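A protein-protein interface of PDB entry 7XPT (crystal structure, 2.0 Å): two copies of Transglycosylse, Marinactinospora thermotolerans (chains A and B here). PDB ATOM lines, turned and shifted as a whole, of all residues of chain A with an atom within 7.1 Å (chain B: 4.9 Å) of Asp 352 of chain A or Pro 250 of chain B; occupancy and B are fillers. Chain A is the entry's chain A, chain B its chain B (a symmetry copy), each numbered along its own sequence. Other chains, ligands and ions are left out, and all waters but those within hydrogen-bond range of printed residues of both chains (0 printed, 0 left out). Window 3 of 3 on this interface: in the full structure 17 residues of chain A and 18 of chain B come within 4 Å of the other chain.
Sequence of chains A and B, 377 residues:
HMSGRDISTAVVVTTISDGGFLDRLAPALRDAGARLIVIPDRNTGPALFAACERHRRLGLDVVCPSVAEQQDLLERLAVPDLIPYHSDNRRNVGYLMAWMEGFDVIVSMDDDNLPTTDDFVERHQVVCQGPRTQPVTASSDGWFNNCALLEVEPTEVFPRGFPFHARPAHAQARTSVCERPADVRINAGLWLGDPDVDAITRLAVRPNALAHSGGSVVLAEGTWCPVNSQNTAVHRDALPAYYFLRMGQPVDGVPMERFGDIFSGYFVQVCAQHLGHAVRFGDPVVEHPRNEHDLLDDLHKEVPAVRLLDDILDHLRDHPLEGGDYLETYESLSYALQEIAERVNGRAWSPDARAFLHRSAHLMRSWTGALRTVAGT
Printed residues of chain A that touch a printed residue of chain B: Pro 250, Pro 351, Asp 352 and Ala 355.
Hydrophobic or aromatic side chains of chain A within 4 Å of the printed part of chain B: Pro 250, Pro 351 and Ala 355.
Among the printed residues, 5 pairs touch across the chains.
Pro 250 of chain A touches Asp 352 of chain B, and with the chains exchanged Asp 352 of chain A touches Pro 250 of chain B.
8 positions are printed for both chains.
Of the 5 pairs that touch across the chains among the printed residues, 2 have their exchanged pair printed and touching as well.
Pro 250 of chain A touches Asp 352 of chain B (CG to CB, 3.6 Å).
CB of Pro 351 of chain A touches O of Gly 248 of chain B (3.6 Å).
Pro 250 of chain B touches Asp 352 of chain A.
Gln 249 of chain B touches Ala 355 of chain A (NE2 to CB, 3.6 Å).
Of the printed residues of chain B, Pro 250 of chain A touches Asp 352 (3.6 Å).
Of the printed residues of chain B, Pro 351 of chain A touches Gly 248 (3.6 Å) and Gln 249 (3.2 Å).
Asp 352 of chain A touches just one residue of chain B: Pro 250.
Of the printed residues of chain B, Ala 355 of chain A touches Gln 249 (3.6 Å).
Printed residues of chain A within 4 Å of Gly 248 of chain B: Pro 351.
Of the printed residues of chain A, Gln 249 of chain B touches Pro 351 and Ala 355.
Of chain A, only Asp 352 comes within 4 Å of Pro 250 of chain B.
The nearest residue of chain B that does not touch Asp 352 of chain A is Gln 249 of chain B (4.3 Å).
The nearest printed residue of chain A that does not touch Asp 352 of chain B is Gln 249 of chain A (4.4 Å).
The side-chain carboxylate (OD2) of Asp 352 of chain A sits at hydrogen-bond distance from the backbone NH (N) of Asp 252 of chain A (3.0 Å).
N of Met 256 of chain B is in hydrogen-bond range of O of Gln 249 of chain B, 3.0 Å away.
The side-chain carboxylate of Asp 352 of chain A is in hydrogen-bond range of the backbone NH of Gly 253 of chain A (3.0 Å).
O of Met 256 of chain B lies within hydrogen-bond range of N of Gly 248 of chain B (2.8 Å).
N of Asp 252 of chain B sits at hydrogen-bond distance from OD2 of Asp 352 of chain B (3.0 Å).
N of Gly 253 of chain B sits at hydrogen-bond distance from OD2 of Asp 352 of chain B, at 3.0 Å.
O of Pro 351 of chain A is in hydrogen-bond range of NE2 of Gln 249 of chain B (3.2 Å).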
ATOM      1  N   GLN A 249      30.681 -24.061 -33.580  1.00  0.00           N
ATOM      2  CA  GLN A 249      30.437 -22.879 -32.762  1.00  0.00           C
ATOM      3  C   GLN A 249      28.940 -22.620 -32.660  1.00  0.00           C
ATOM      4  O   GLN A 249      28.239 -22.649 -33.679  1.00  0.00           O
ATOM      5  CB  GLN A 249      31.143 -21.661 -33.355  1.00  0.00           C
ATOM      6  CG  GLN A 249      32.661 -21.711 -33.269  1.00  0.00           C
ATOM      7  CD  GLN A 249      33.167 -21.598 -31.845  1.00  0.00           C
ATOM      8  OE1 GLN A 249      34.196 -22.173 -31.496  1.00  0.00           O
ATOM      9  NE2 GLN A 249      32.443 -20.853 -31.014  1.00  0.00           N
ATOM     10  N   PRO A 250      28.412 -22.365 -31.467  1.00  0.00           N
ATOM     11  CA  PRO A 250      26.978 -22.104 -31.334  1.00  0.00           C
ATOM     12  C   PRO A 250      26.608 -20.676 -31.703  1.00  0.00           C
ATOM     13  O   PRO A 250      27.374 -19.729 -31.505  1.00  0.00           O
ATOM     14  CB  PRO A 250      26.713 -22.368 -29.847  1.00  0.00           C
ATOM     15  CG  PRO A 250      28.000 -22.024 -29.189  1.00  0.00           C
ATOM     16  CD  PRO A 250      29.085 -22.432 -30.158  1.00  0.00           C
ATOM     17  N   VAL A 251      25.407 -20.539 -32.255  1.00  0.00           N
ATOM     18  CA  VAL A 251      24.788 -19.247 -32.526  1.00  0.00           C
ATOM     19  C   VAL A 251      23.448 -19.257 -31.808  1.00  0.00           C
ATOM     20  O   VAL A 251      22.531 -19.990 -32.205  1.00  0.00           O
ATOM     21  CB  VAL A 251      24.613 -18.987 -34.028  1.00  0.00           C
ATOM     22  CG1 VAL A 251      23.978 -17.622 -34.260  1.00  0.00           C
ATOM     23  CG2 VAL A 251      25.948 -19.090 -34.743  1.00  0.00           C
ATOM     24  N   ASP A 252      23.336 -18.456 -30.747  1.00  0.00           N
ATOM     25  CA  ASP A 252      22.185 -18.503 -29.844  1.00  0.00           C
ATOM     26  C   ASP A 252      21.991 -19.909 -29.281  1.00  0.00           C
ATOM     27  O   ASP A 252      20.865 -20.368 -29.073  1.00  0.00           O
ATOM     28  CB  ASP A 252      20.909 -18.006 -30.532  1.00  0.00           C
ATOM     29  CG  ASP A 252      20.745 -16.504 -30.440  1.00  0.00           C
ATOM     30  OD1 ASP A 252      21.492 -15.774 -31.127  1.00  0.00           O
ATOM     31  OD2 ASP A 252      19.867 -16.051 -29.675  1.00  0.00           O
ATOM     32  N   GLY A 253      23.102 -20.601 -29.041  1.00  0.00           N
ATOM     33  CA  GLY A 253      23.070 -21.927 -28.463  1.00  0.00           C
ATOM     34  C   GLY A 253      22.858 -23.064 -29.438  1.00  0.00           C
ATOM     35  O   GLY A 253      22.613 -24.192 -28.996  1.00  0.00           O
ATOM     36  N   VAL A 254      22.939 -22.811 -30.740  1.00  0.00           N
ATOM     37  CA  VAL A 254      22.752 -23.835 -31.758  1.00  0.00           C
ATOM     38  C   VAL A 254      24.066 -23.986 -32.516  1.00  0.00           C
ATOM     39  O   VAL A 254      24.502 -23.046 -33.185  1.00  0.00           O
ATOM     40  CB  VAL A 254      21.607 -23.490 -32.725  1.00  0.00           C
ATOM     41  CG1 VAL A 254      21.199 -24.720 -33.530  1.00  0.00           C
ATOM     42  CG2 VAL A 254      20.420 -22.923 -31.962  1.00  0.00           C
ATOM     43  N   LEU A 308      24.016 -15.582 -40.033  1.00  0.00           N
ATOM     44  CA  LEU A 308      25.076 -14.593 -39.912  1.00  0.00           C
ATOM     45  C   LEU A 308      25.761 -14.265 -41.231  1.00  0.00           C
ATOM     46  O   LEU A 308      26.466 -13.253 -41.305  1.00  0.00           O
ATOM     47  CB  LEU A 308      26.140 -15.077 -38.914  1.00  0.00           C
ATOM     48  CG  LEU A 308      25.666 -15.638 -37.570  1.00  0.00           C
ATOM     49  CD1 LEU A 308      26.851 -16.198 -36.797  1.00  0.00           C
ATOM     50  CD2 LEU A 308      24.954 -14.569 -36.756  1.00  0.00           C
ATOM     51  N   ALA A 348      20.504 -11.921 -34.450  1.00  0.00           N
ATOM     52  CA  ALA A 348      21.270 -13.159 -34.438  1.00  0.00           C
ATOM     53  C   ALA A 348      22.668 -12.994 -33.862  1.00  0.00           C
ATOM     54  O   ALA A 348      23.368 -13.996 -33.687  1.00  0.00           O
ATOM     55  CB  ALA A 348      21.368 -13.730 -35.855  1.00  0.00           C
ATOM     56  N   TRP A 349      23.095 -11.767 -33.564  1.00  0.00           N
ATOM     57  CA  TRP A 349      24.456 -11.522 -33.088  1.00  0.00           C
ATOM     58  C   TRP A 349      24.474 -11.472 -31.561  1.00  0.00           C
ATOM     59  O   TRP A 349      24.657 -10.430 -30.929  1.00  0.00           O
ATOM     60  CB  TRP A 349      25.016 -10.246 -33.713  1.00  0.00           C
ATOM     61  CG  TRP A 349      25.302 -10.413 -35.171  1.00  0.00           C
ATOM     62  CD1 TRP A 349      24.556  -9.947 -36.212  1.00  0.00           C
ATOM     63  CD2 TRP A 349      26.398 -11.133 -35.751  1.00  0.00           C
ATOM     64  NE1 TRP A 349      25.128 -10.317 -37.406  1.00  0.00           N
ATOM     65  CE2 TRP A 349      26.258 -11.048 -37.150  1.00  0.00           C
ATOM     66  CE3 TRP A 349      27.485 -11.835 -35.222  1.00  0.00           C
ATOM     67  CZ2 TRP A 349      27.167 -11.636 -38.028  1.00  0.00           C
ATOM     68  CZ3 TRP A 349      28.388 -12.418 -36.097  1.00  0.00           C
ATOM     69  CH2 TRP A 349      28.223 -12.314 -37.483  1.00  0.00           C
ATOM     70  N   SER A 350      24.273 -12.647 -30.976  1.00  0.00           N
ATOM     71  CA  SER A 350      24.423 -12.845 -29.545  1.00  0.00           C
ATOM     72  C   SER A 350      25.905 -12.924 -29.197  1.00  0.00           C
ATOM     73  O   SER A 350      26.757 -13.015 -30.084  1.00  0.00           O
ATOM     74  CB  SER A 350      23.676 -14.110 -29.127  1.00  0.00           C
ATOM     75  OG  SER A 350      24.062 -15.207 -29.932  1.00  0.00           O
ATOM     76  N   PRO A 351      26.253 -12.867 -27.906  1.00  0.00           N
ATOM     77  CA  PRO A 351      27.676 -12.955 -27.536  1.00  0.00           C
ATOM     78  C   PRO A 351      28.388 -14.193 -28.061  1.00  0.00           C
ATOM     79  O   PRO A 351      29.595 -14.126 -28.322  1.00  0.00           O
ATOM     80  CB  PRO A 351      27.631 -12.934 -26.003  1.00  0.00           C
ATOM     81  CG  PRO A 351      26.438 -12.112 -25.697  1.00  0.00           C
ATOM     82  CD  PRO A 351      25.423 -12.448 -26.761  1.00  0.00           C
ATOM     83  N   ASP A 352      27.695 -15.323 -28.226  1.00  0.00           N
ATOM     84  CA  ASP A 352      28.372 -16.487 -28.788  1.00  0.00           C
ATOM     85  C   ASP A 352      28.535 -16.372 -30.299  1.00  0.00           C
ATOM     86  O   ASP A 352      29.507 -16.899 -30.852  1.00  0.00           O
ATOM     87  CB  ASP A 352      27.639 -17.783 -28.420  1.00  0.00           C
ATOM     88  CG  ASP A 352      26.176 -17.792 -28.845  1.00  0.00           C
ATOM     89  OD1 ASP A 352      25.673 -16.758 -29.325  1.00  0.00           O
ATOM     90  OD2 ASP A 352      25.527 -18.849 -28.690  1.00  0.00           O
ATOM     91  N   ALA A 353      27.616 -15.682 -30.977  1.00  0.00           N
ATOM     92  CA  ALA A 353      27.779 -15.445 -32.408  1.00  0.00           C
ATOM     93  C   ALA A 353      28.984 -14.555 -32.686  1.00  0.00           C
ATOM     94  O   ALA A 353      29.719 -14.777 -33.656  1.00  0.00           O
ATOM     95  CB  ALA A 353      26.508 -14.821 -32.985  1.00  0.00           C
ATOM     96  N   ARG A 354      29.201 -13.539 -31.846  1.00  0.00           N
ATOM     97  CA  ARG A 354      30.358 -12.672 -32.027  1.00  0.00           C
ATOM     98  C   ARG A 354      31.650 -13.404 -31.692  1.00  0.00           C
ATOM     99  O   ARG A 354      32.653 -13.266 -32.403  1.00  0.00           O
ATOM    100  CB  ARG A 354      30.211 -11.418 -31.165  1.00  0.00           C
ATOM    101  CG  ARG A 354      28.935 -10.632 -31.421  1.00  0.00           C
ATOM    102  CD  ARG A 354      28.875  -9.391 -30.549  1.00  0.00           C
ATOM    103  NE  ARG A 354      27.659  -8.617 -30.772  1.00  0.00           N
ATOM    104  CZ  ARG A 354      27.542  -7.650 -31.671  1.00  0.00           C
ATOM    105  NH1 ARG A 354      28.552  -7.314 -32.458  1.00  0.00           N
ATOM    106  NH2 ARG A 354      26.385  -7.003 -31.782  1.00  0.00           N
ATOM    107  N   ALA A 355      31.645 -14.194 -30.615  1.00  0.00           N
ATOM    108  CA  ALA A 355      32.829 -14.957 -30.240  1.00  0.00           C
ATOM    109  C   ALA A 355      33.178 -16.026 -31.266  1.00  0.00           C
ATOM    110  O   ALA A 355      34.322 -16.491 -31.290  1.00  0.00           O
ATOM    111  CB  ALA A 355      32.626 -15.593 -28.864  1.00  0.00           C
ATOM    112  N   PHE A 356      32.221 -16.426 -32.107  1.00  0.00           N
ATOM    113  CA  PHE A 356      32.527 -17.363 -33.185  1.00  0.00           C
ATOM    114  C   PHE A 356      33.567 -16.788 -34.138  1.00  0.00           C
ATOM    115  O   PHE A 356      34.501 -17.487 -34.548  1.00  0.00           O
ATOM    116  CB  PHE A 356      31.245 -17.729 -33.937  1.00  0.00           C
ATOM    117  CG  PHE A 356      31.458 -18.038 -35.392  1.00  0.00           C
ATOM    118  CD1 PHE A 356      32.060 -19.222 -35.787  1.00  0.00           C
ATOM    119  CD2 PHE A 356      31.042 -17.147 -36.370  1.00  0.00           C
ATOM    120  CE1 PHE A 356      32.256 -19.507 -37.127  1.00  0.00           C
ATOM    121  CE2 PHE A 356      31.232 -17.427 -37.712  1.00  0.00           C
ATOM    122  CZ  PHE A 356      31.838 -18.608 -38.089  1.00  0.00           C
ATOM    123  N   LEU A 357      33.424 -15.512 -34.502  1.00  0.00           N
ATOM    124  CA  LEU A 357      34.404 -14.888 -35.387  1.00  0.00           C
ATOM    125  C   LEU A 357      35.748 -14.709 -34.698  1.00  0.00           C
ATOM    126  O   LEU A 357      36.792 -14.769 -35.357  1.00  0.00           O
ATOM    127  CB  LEU A 357      33.878 -13.543 -35.887  1.00  0.00           C
ATOM    128  CG  LEU A 357      32.699 -13.601 -36.862  1.00  0.00           C
ATOM    129  CD1 LEU A 357      32.108 -12.215 -37.098  1.00  0.00           C
ATOM    130  CD2 LEU A 357      33.131 -14.234 -38.178  1.00  0.00           C
ATOM    131  N   GLY B 248      28.668 -11.868 -19.927  1.00  0.00           N
ATOM    132  CA  GLY B 248      27.617 -12.255 -20.842  1.00  0.00           C
ATOM    133  C   GLY B 248      27.973 -13.368 -21.800  1.00  0.00           C
ATOM    134  O   GLY B 248      27.099 -13.812 -22.555  1.00  0.00           O
ATOM    135  N   GLN B 249      29.217 -13.834 -21.800  1.00  0.00           N
ATOM    136  CA  GLN B 249      29.602 -14.913 -22.703  1.00  0.00           C
ATOM    137  C   GLN B 249      29.053 -16.238 -22.192  1.00  0.00           C
ATOM    138  O   GLN B 249      29.240 -16.567 -21.016  1.00  0.00           O
ATOM    139  CB  GLN B 249      31.118 -14.994 -22.841  1.00  0.00           C
ATOM    140  CG  GLN B 249      31.739 -13.825 -23.588  1.00  0.00           C
ATOM    141  CD  GLN B 249      31.302 -13.765 -25.037  1.00  0.00           C
ATOM    142  OE1 GLN B 249      31.128 -12.683 -25.597  1.00  0.00           O
ATOM    143  NE2 GLN B 249      31.126 -14.930 -25.654  1.00  0.00           N
ATOM    144  N   PRO B 250      28.380 -17.019 -23.031  1.00  0.00           N
ATOM    145  CA  PRO B 250      27.801 -18.277 -22.550  1.00  0.00           C
ATOM    146  C   PRO B 250      28.858 -19.349 -22.343  1.00  0.00           C
ATOM    147  O   PRO B 250      29.843 -19.437 -23.081  1.00  0.00           O
ATOM    148  CB  PRO B 250      26.822 -18.664 -23.665  1.00  0.00           C
ATOM    149  CG  PRO B 250      27.406 -18.054 -24.885  1.00  0.00           C
ATOM    150  CD  PRO B 250      28.037 -16.755 -24.439  1.00  0.00           C
ATOM    151  N   VAL B 251      28.647 -20.155 -21.308  1.00  0.00           N
ATOM    152  CA  VAL B 251      29.382 -21.393 -21.081  1.00  0.00           C
ATOM    153  C   VAL B 251      28.340 -22.499 -21.068  1.00  0.00           C
ATOM    154  O   VAL B 251      27.515 -22.567 -20.149  1.00  0.00           O
ATOM    155  CB  VAL B 251      30.180 -21.371 -19.770  1.00  0.00           C
ATOM    156  CG1 VAL B 251      30.888 -22.704 -19.558  1.00  0.00           C
ATOM    157  CG2 VAL B 251      31.174 -20.227 -19.773  1.00  0.00           C
ATOM    158  N   ASP B 252      28.363 -23.352 -22.094  1.00  0.00           N
ATOM    159  CA  ASP B 252      27.328 -24.365 -22.295  1.00  0.00           C
ATOM    160  C   ASP B 252      25.946 -23.722 -22.392  1.00  0.00           C
ATOM    161  O   ASP B 252      24.962 -24.236 -21.857  1.00  0.00           O
ATOM    162  CB  ASP B 252      27.357 -25.429 -21.195  1.00  0.00           C
ATOM    163  CG  ASP B 252      28.363 -26.525 -21.473  1.00  0.00           C
ATOM    164  OD1 ASP B 252      29.579 -26.233 -21.479  1.00  0.00           O
ATOM    165  OD2 ASP B 252      27.937 -27.679 -21.683  1.00  0.00           O
ATOM    166  N   GLY B 253      25.877 -22.581 -23.073  1.00  0.00           N
ATOM    167  CA  GLY B 253      24.620 -21.885 -23.256  1.00  0.00           C
ATOM    168  C   GLY B 253      24.128 -21.109 -22.056  1.00  0.00           C
ATOM    169  O   GLY B 253      22.979 -20.653 -22.069  1.00  0.00           O
ATOM    170  N   VAL B 254      24.945 -20.947 -21.026  1.00  0.00           N
ATOM    171  CA  VAL B 254      24.575 -20.208 -19.822  1.00  0.00           C
ATOM    172  C   VAL B 254      25.461 -18.970 -19.740  1.00  0.00           C
ATOM    173  O   VAL B 254      26.683 -19.100 -19.599  1.00  0.00           O
ATOM    174  CB  VAL B 254      24.718 -21.070 -18.557  1.00  0.00           C
ATOM    175  CG1 VAL B 254      23.992 -20.416 -17.391  1.00  0.00           C
ATOM    176  CG2 VAL B 254      24.189 -22.479 -18.808  1.00  0.00           C
ATOM    177  N   PRO B 255      24.900 -17.763 -19.812  1.00  0.00           N
ATOM    178  CA  PRO B 255      25.741 -16.557 -19.822  1.00  0.00           C
ATOM    179  C   PRO B 255      26.380 -16.311 -18.462  1.00  0.00           C
ATOM    180  O   PRO B 255      25.712 -16.353 -17.428  1.00  0.00           O
ATOM    181  CB  PRO B 255      24.755 -15.444 -20.194  1.00  0.00           C
ATOM    182  CG  PRO B 255      23.425 -15.955 -19.727  1.00  0.00           C
ATOM    183  CD  PRO B 255      23.465 -17.446 -19.921  1.00  0.00           C
ATOM    184  N   MET B 256      27.683 -16.050 -18.469  1.00  0.00           N
ATOM    185  CA  MET B 256      28.390 -15.763 -17.232  1.00  0.00           C
ATOM    186  C   MET B 256      28.198 -14.305 -16.830  1.00  0.00           C
ATOM    187  O   MET B 256      27.952 -13.432 -17.668  1.00  0.00           O
ATOM    188  CB  MET B 256      29.881 -16.068 -17.376  1.00  0.00           C
ATOM    189  CG  MET B 256      30.614 -15.113 -18.299  1.00  0.00           C
ATOM    190  SD  MET B 256      32.405 -15.217 -18.125  1.00  0.00           S
ATOM    191  CE  MET B 256      32.710 -16.882 -18.711  1.00  0.00           C
ATOM    192  N   ASP B 352      31.743 -22.736 -27.058  1.00  0.00           N
ATOM    193  CA  ASP B 352      31.475 -21.373 -26.613  1.00  0.00           C
ATOM    194  C   ASP B 352      32.322 -20.977 -25.412  1.00  0.00           C
ATOM    195  O   ASP B 352      32.570 -19.783 -25.212  1.00  0.00           O
ATOM    196  CB  ASP B 352      29.986 -21.186 -26.298  1.00  0.00           C
ATOM    197  CG  ASP B 352      29.475 -22.139 -25.226  1.00  0.00           C
ATOM    198  OD1 ASP B 352      30.232 -23.033 -24.795  1.00  0.00           O
ATOM    199  OD2 ASP B 352      28.303 -21.992 -24.816  1.00  0.00           O
ATOM    200  N   ALA B 353      32.783 -21.946 -24.620  1.00  0.00           N
ATOM    201  CA  ALA B 353      33.695 -21.628 -23.527  1.00  0.00           C
ATOM    202  C   ALA B 353      35.061 -21.214 -24.056  1.00  0.00           C
ATOM    203  O   ALA B 353      35.644 -20.230 -23.585  1.00  0.00           O
ATOM    204  CB  ALA B 353      33.822 -22.823 -22.584  1.00  0.00           C
